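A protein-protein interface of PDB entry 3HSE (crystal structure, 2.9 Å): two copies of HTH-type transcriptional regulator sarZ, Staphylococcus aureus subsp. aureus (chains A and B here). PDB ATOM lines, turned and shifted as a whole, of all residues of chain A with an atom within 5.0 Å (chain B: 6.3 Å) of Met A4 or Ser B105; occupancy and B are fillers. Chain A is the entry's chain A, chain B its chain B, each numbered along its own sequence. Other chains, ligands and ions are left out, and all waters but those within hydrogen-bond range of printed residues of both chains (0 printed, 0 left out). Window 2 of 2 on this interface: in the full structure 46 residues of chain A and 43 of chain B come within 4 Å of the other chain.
Val B112 touches His A3. Met A4 touches Ser B105. Met A4 touches Ala B108 (CE to CB, 3.3 Å). CA of Met A4 touches CG2 of Val B112 (3.8 Å). Leu A6 touches Glu B122. Ser A7 touches Val B112.
Of the 8 printed residues of chain A, 5 touch a printed residue of chain B. Printed residues of chain A that touch a printed residue of chain B: Ser A2, His A3, Met A4, Leu A6 and Ser A7. Hydrophobic or aromatic side chains of chain A that line the printed part of chain B: His A3, Met A4 and Leu A6. Among the printed residues, 9 pairs touch across the chains.
No position is printed for both chains. Of the 9 pairs that touch across the chains among the printed residues, none has its exchanged pair printed and touching as well.
The side-chain hydroxyl of Ser A2 sits at hydrogen-bond distance from the side-chain carboxylate of Glu B122, 2.6 Å away. The side-chain carboxylate (OE2) of Glu B122 sits close to a ring nitrogen (NE2) of His A3 (3.2 Å). OG of Ser A7 sits close to O of Ser B111 (3.4 Å).
Of chain B, only Ser B105 (3.6 Å), Ala B108 (3.3 Å) and Val B112 (3.8 Å) come within 4 Å of Met A4. Of the printed residues of chain A, Ser B105 touches Met A4. Printed residues of chain B within 4 Å of His A3: Val B112 and Glu B122. Of the printed residues of chain B, Leu A6 touches Glu B122. Ile B103 touches none of the printed residues of chain A. Lys B104 touches none of the printed residues of chain A. The nearest printed residue of chain B that does not touch Ser A2 is Val B112 (6.9 Å).
OG of Ser A7 lies within hydrogen-bond range of O of His A3, 2.7 Å away.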
ATOM      1  N   GLY A   1     -13.267  -9.918  15.288  1.00  0.00           N
ATOM      2  CA  GLY A   1     -14.418  -9.363  14.537  1.00  0.00           C
ATOM      3  C   GLY A   1     -15.140 -10.397  13.691  1.00  0.00           C
ATOM      4  O   GLY A   1     -15.592 -11.422  14.199  1.00  0.00           O
ATOM      5  N   SER A   2     -15.244 -10.131  12.392  1.00  0.00           N
ATOM      6  CA  SER A   2     -15.923 -11.035  11.465  1.00  0.00           C
ATOM      7  C   SER A   2     -15.266 -12.403  11.363  1.00  0.00           C
ATOM      8  O   SER A   2     -15.960 -13.415  11.325  1.00  0.00           O
ATOM      9  CB  SER A   2     -15.987 -10.422  10.071  1.00  0.00           C
ATOM     10  OG  SER A   2     -14.718 -10.505   9.451  1.00  0.00           O
ATOM     11  N   HIS A   3     -13.940 -12.451  11.295  1.00  0.00           N
ATOM     12  CA  HIS A   3     -13.282 -13.743  11.205  1.00  0.00           C
ATOM     13  C   HIS A   3     -13.574 -14.499  12.503  1.00  0.00           C
ATOM     14  O   HIS A   3     -13.795 -15.713  12.507  1.00  0.00           O
ATOM     15  CB  HIS A   3     -11.777 -13.573  10.979  1.00  0.00           C
ATOM     16  CG  HIS A   3     -11.419 -13.020   9.631  1.00  0.00           C
ATOM     17  ND1 HIS A   3     -11.204 -11.677   9.404  1.00  0.00           N
ATOM     18  CD2 HIS A   3     -11.238 -13.630   8.431  1.00  0.00           C
ATOM     19  CE1 HIS A   3     -10.903 -11.481   8.129  1.00  0.00           C
ATOM     20  NE2 HIS A   3     -10.919 -12.653   7.519  1.00  0.00           N
ATOM     21  N   MET A   4     -13.608 -13.762  13.608  1.00  0.00           N
ATOM     22  CA  MET A   4     -13.898 -14.349  14.915  1.00  0.00           C
ATOM     23  C   MET A   4     -15.349 -14.821  14.905  1.00  0.00           C
ATOM     24  O   MET A   4     -15.663 -15.923  15.352  1.00  0.00           O
ATOM     25  CB  MET A   4     -13.718 -13.302  16.012  1.00  0.00           C
ATOM     26  CG  MET A   4     -13.171 -13.837  17.316  1.00  0.00           C
ATOM     27  SD  MET A   4     -11.781 -12.787  17.882  1.00  0.00           S
ATOM     28  CE  MET A   4     -11.838 -13.079  19.646  1.00  0.00           C
ATOM     29  N   TYR A   5     -16.227 -13.971  14.384  1.00  0.00           N
ATOM     30  CA  TYR A   5     -17.643 -14.275  14.325  1.00  0.00           C
ATOM     31  C   TYR A   5     -17.945 -15.542  13.546  1.00  0.00           C
ATOM     32  O   TYR A   5     -18.631 -16.429  14.044  1.00  0.00           O
ATOM     33  CB  TYR A   5     -18.423 -13.108  13.714  1.00  0.00           C
ATOM     34  CG  TYR A   5     -19.907 -13.382  13.656  1.00  0.00           C
ATOM     35  CD1 TYR A   5     -20.666 -13.446  14.828  1.00  0.00           C
ATOM     36  CD2 TYR A   5     -20.530 -13.691  12.441  1.00  0.00           C
ATOM     37  CE1 TYR A   5     -22.008 -13.826  14.796  1.00  0.00           C
ATOM     38  CE2 TYR A   5     -21.873 -14.071  12.393  1.00  0.00           C
ATOM     39  CZ  TYR A   5     -22.607 -14.140  13.579  1.00  0.00           C
ATOM     40  OH  TYR A   5     -23.930 -14.535  13.549  1.00  0.00           O
ATOM     41  N   LEU A   6     -17.432 -15.633  12.327  1.00  0.00           N
ATOM     42  CA  LEU A   6     -17.677 -16.809  11.497  1.00  0.00           C
ATOM     43  C   LEU A   6     -17.123 -18.112  12.067  1.00  0.00           C
ATOM     44  O   LEU A   6     -17.770 -19.156  11.944  1.00  0.00           O
ATOM     45  CB  LEU A   6     -17.111 -16.601  10.101  1.00  0.00           C
ATOM     46  CG  LEU A   6     -17.731 -15.463   9.297  1.00  0.00           C
ATOM     47  CD1 LEU A   6     -16.866 -15.235   8.087  1.00  0.00           C
ATOM     48  CD2 LEU A   6     -19.158 -15.768   8.893  1.00  0.00           C
ATOM     49  N   SER A   7     -15.939 -18.055  12.681  1.00  0.00           N
ATOM     50  CA  SER A   7     -15.312 -19.246  13.258  1.00  0.00           C
ATOM     51  C   SER A   7     -16.224 -19.775  14.345  1.00  0.00           C
ATOM     52  O   SER A   7     -16.544 -20.969  14.408  1.00  0.00           O
ATOM     53  CB  SER A   7     -13.950 -18.900  13.868  1.00  0.00           C
ATOM     54  OG  SER A   7     -13.119 -18.249  12.929  1.00  0.00           O
ATOM     55  N   LYS A   8     -16.611 -18.855  15.214  1.00  0.00           N
ATOM     56  CA  LYS A   8     -17.516 -19.121  16.307  1.00  0.00           C
ATOM     57  C   LYS A   8     -18.656 -19.920  15.665  1.00  0.00           C
ATOM     58  O   LYS A   8     -18.861 -21.080  15.984  1.00  0.00           O
ATOM     59  CB  LYS A   8     -18.009 -17.776  16.827  1.00  0.00           C
ATOM     60  CG  LYS A   8     -18.464 -17.710  18.261  1.00  0.00           C
ATOM     61  CD  LYS A   8     -19.230 -16.397  18.444  1.00  0.00           C
ATOM     62  CE  LYS A   8     -19.806 -16.257  19.853  1.00  0.00           C
ATOM     63  NZ  LYS A   8     -20.526 -14.959  20.035  1.00  0.00           N
ATOM     64  N   LYS B 101     -13.514 -15.145  32.282  1.00  0.00           N
ATOM     65  CA  LYS B 101     -13.918 -14.086  31.352  1.00  0.00           C
ATOM     66  C   LYS B 101     -12.717 -13.393  30.732  1.00  0.00           C
ATOM     67  O   LYS B 101     -12.857 -12.655  29.751  1.00  0.00           O
ATOM     68  CB  LYS B 101     -14.760 -13.020  32.055  1.00  0.00           C
ATOM     69  CG  LYS B 101     -16.090 -13.475  32.621  1.00  0.00           C
ATOM     70  CD  LYS B 101     -16.802 -12.276  33.232  1.00  0.00           C
ATOM     71  CE  LYS B 101     -18.146 -12.633  33.832  1.00  0.00           C
ATOM     72  NZ  LYS B 101     -18.880 -11.390  34.207  1.00  0.00           N
ATOM     73  N   ALA B 102     -11.543 -13.628  31.313  1.00  0.00           N
ATOM     74  CA  ALA B 102     -10.305 -13.014  30.837  1.00  0.00           C
ATOM     75  C   ALA B 102      -9.829 -13.634  29.533  1.00  0.00           C
ATOM     76  O   ALA B 102      -9.375 -12.933  28.623  1.00  0.00           O
ATOM     77  CB  ALA B 102      -9.220 -13.155  31.901  1.00  0.00           C
ATOM     78  N   ILE B 103      -9.945 -14.953  29.455  1.00  0.00           N
ATOM     79  CA  ILE B 103      -9.507 -15.698  28.290  1.00  0.00           C
ATOM     80  C   ILE B 103     -10.567 -15.907  27.203  1.00  0.00           C
ATOM     81  O   ILE B 103     -10.362 -16.705  26.286  1.00  0.00           O
ATOM     82  CB  ILE B 103      -8.956 -17.063  28.711  1.00  0.00           C
ATOM     83  CG1 ILE B 103      -9.946 -17.750  29.639  1.00  0.00           C
ATOM     84  CG2 ILE B 103      -7.641 -16.895  29.430  1.00  0.00           C
ATOM     85  CD1 ILE B 103      -9.551 -19.164  30.001  1.00  0.00           C
ATOM     86  N   LYS B 104     -11.688 -15.193  27.301  1.00  0.00           N
ATOM     87  CA  LYS B 104     -12.749 -15.298  26.305  1.00  0.00           C
ATOM     88  C   LYS B 104     -12.192 -14.946  24.921  1.00  0.00           C
ATOM     89  O   LYS B 104     -12.582 -15.525  23.899  1.00  0.00           O
ATOM     90  CB  LYS B 104     -13.900 -14.340  26.643  1.00  0.00           C
ATOM     91  CG  LYS B 104     -14.958 -14.265  25.542  1.00  0.00           C
ATOM     92  CD  LYS B 104     -15.941 -13.109  25.701  1.00  0.00           C
ATOM     93  CE  LYS B 104     -16.820 -12.995  24.445  1.00  0.00           C
ATOM     94  NZ  LYS B 104     -17.981 -12.054  24.574  1.00  0.00           N
ATOM     95  N   SER B 105     -11.273 -13.989  24.911  1.00  0.00           N
ATOM     96  CA  SER B 105     -10.639 -13.517  23.689  1.00  0.00           C
ATOM     97  C   SER B 105      -9.674 -14.559  23.090  1.00  0.00           C
ATOM     98  O   SER B 105      -9.799 -14.940  21.918  1.00  0.00           O
ATOM     99  CB  SER B 105      -9.904 -12.208  23.987  1.00  0.00           C
ATOM    100  OG  SER B 105      -9.442 -11.598  22.799  1.00  0.00           O
ATOM    101  N   PRO B 106      -8.687 -15.020  23.879  1.00  0.00           N
ATOM    102  CA  PRO B 106      -7.753 -16.021  23.345  1.00  0.00           C
ATOM    103  C   PRO B 106      -8.448 -17.346  22.986  1.00  0.00           C
ATOM    104  O   PRO B 106      -8.015 -18.047  22.079  1.00  0.00           O
ATOM    105  CB  PRO B 106      -6.732 -16.171  24.470  1.00  0.00           C
ATOM    106  CG  PRO B 106      -7.532 -15.846  25.696  1.00  0.00           C
ATOM    107  CD  PRO B 106      -8.316 -14.647  25.256  1.00  0.00           C
ATOM    108  N   LEU B 107      -9.515 -17.688  23.705  1.00  0.00           N
ATOM    109  CA  LEU B 107     -10.259 -18.910  23.424  1.00  0.00           C
ATOM    110  C   LEU B 107     -10.995 -18.775  22.103  1.00  0.00           C
ATOM    111  O   LEU B 107     -10.977 -19.682  21.266  1.00  0.00           O
ATOM    112  CB  LEU B 107     -11.275 -19.191  24.522  1.00  0.00           C
ATOM    113  CG  LEU B 107     -10.669 -19.692  25.822  1.00  0.00           C
ATOM    114  CD1 LEU B 107     -11.794 -20.188  26.721  1.00  0.00           C
ATOM    115  CD2 LEU B 107      -9.672 -20.819  25.541  1.00  0.00           C
ATOM    116  N   ALA B 108     -11.665 -17.642  21.933  1.00  0.00           N
ATOM    117  CA  ALA B 108     -12.394 -17.364  20.709  1.00  0.00           C
ATOM    118  C   ALA B 108     -11.393 -17.460  19.565  1.00  0.00           C
ATOM    119  O   ALA B 108     -11.662 -18.054  18.508  1.00  0.00           O
ATOM    120  CB  ALA B 108     -12.976 -15.969  20.769  1.00  0.00           C
ATOM    121  N   GLU B 109     -10.223 -16.876  19.802  1.00  0.00           N
ATOM    122  CA  GLU B 109      -9.152 -16.861  18.818  1.00  0.00           C
ATOM    123  C   GLU B 109      -8.832 -18.256  18.290  1.00  0.00           C
ATOM    124  O   GLU B 109      -8.457 -18.415  17.120  1.00  0.00           O
ATOM    125  CB  GLU B 109      -7.898 -16.242  19.436  1.00  0.00           C
ATOM    126  CG  GLU B 109      -7.352 -15.100  18.639  1.00  0.00           C
ATOM    127  CD  GLU B 109      -7.324 -15.416  17.174  1.00  0.00           C
ATOM    128  OE1 GLU B 109      -6.662 -16.401  16.802  1.00  0.00           O
ATOM    129  OE2 GLU B 109      -7.966 -14.688  16.391  1.00  0.00           O
ATOM    130  N   ILE B 110      -8.988 -19.260  19.152  1.00  0.00           N
ATOM    131  CA  ILE B 110      -8.712 -20.637  18.766  1.00  0.00           C
ATOM    132  C   ILE B 110      -9.578 -21.123  17.607  1.00  0.00           C
ATOM    133  O   ILE B 110      -9.143 -21.959  16.832  1.00  0.00           O
ATOM    134  CB  ILE B 110      -8.904 -21.612  19.936  1.00  0.00           C
ATOM    135  CG1 ILE B 110      -7.924 -21.273  21.055  1.00  0.00           C
ATOM    136  CG2 ILE B 110      -8.718 -23.046  19.443  1.00  0.00           C
ATOM    137  CD1 ILE B 110      -7.951 -22.224  22.194  1.00  0.00           C
ATOM    138  N   SER B 111     -10.802 -20.613  17.497  1.00  0.00           N
ATOM    139  CA  SER B 111     -11.686 -21.013  16.406  1.00  0.00           C
ATOM    140  C   SER B 111     -11.190 -20.440  15.077  1.00  0.00           C
ATOM    141  O   SER B 111     -11.473 -20.985  14.001  1.00  0.00           O
ATOM    142  CB  SER B 111     -13.117 -20.536  16.672  1.00  0.00           C
ATOM    143  OG  SER B 111     -13.685 -21.213  17.782  1.00  0.00           O
ATOM    144  N   VAL B 112     -10.442 -19.341  15.151  1.00  0.00           N
ATOM    145  CA  VAL B 112      -9.921 -18.708  13.946  1.00  0.00           C
ATOM    146  C   VAL B 112      -8.713 -19.481  13.430  1.00  0.00           C
ATOM    147  O   VAL B 112      -8.605 -19.730  12.240  1.00  0.00           O
ATOM    148  CB  VAL B 112      -9.566 -17.223  14.205  1.00  0.00           C
ATOM    149  CG1 VAL B 112      -9.150 -16.550  12.914  1.00  0.00           C
ATOM    150  CG2 VAL B 112     -10.770 -16.505  14.762  1.00  0.00           C
ATOM    151  N   GLU B 122     -13.605 -16.477   4.311  1.00  0.00           N
ATOM    152  CA  GLU B 122     -14.848 -16.118   4.973  1.00  0.00           C
ATOM    153  C   GLU B 122     -15.979 -16.402   3.995  1.00  0.00           C
ATOM    154  O   GLU B 122     -17.160 -16.326   4.342  1.00  0.00           O
ATOM    155  CB  GLU B 122     -14.846 -14.642   5.361  1.00  0.00           C
ATOM    156  CG  GLU B 122     -13.831 -14.300   6.444  1.00  0.00           C
ATOM    157  CD  GLU B 122     -13.902 -12.845   6.875  1.00  0.00           C
ATOM    158  OE1 GLU B 122     -13.807 -11.953   6.002  1.00  0.00           O
ATOM    159  OE2 GLU B 122     -14.049 -12.593   8.090  1.00  0.00           O
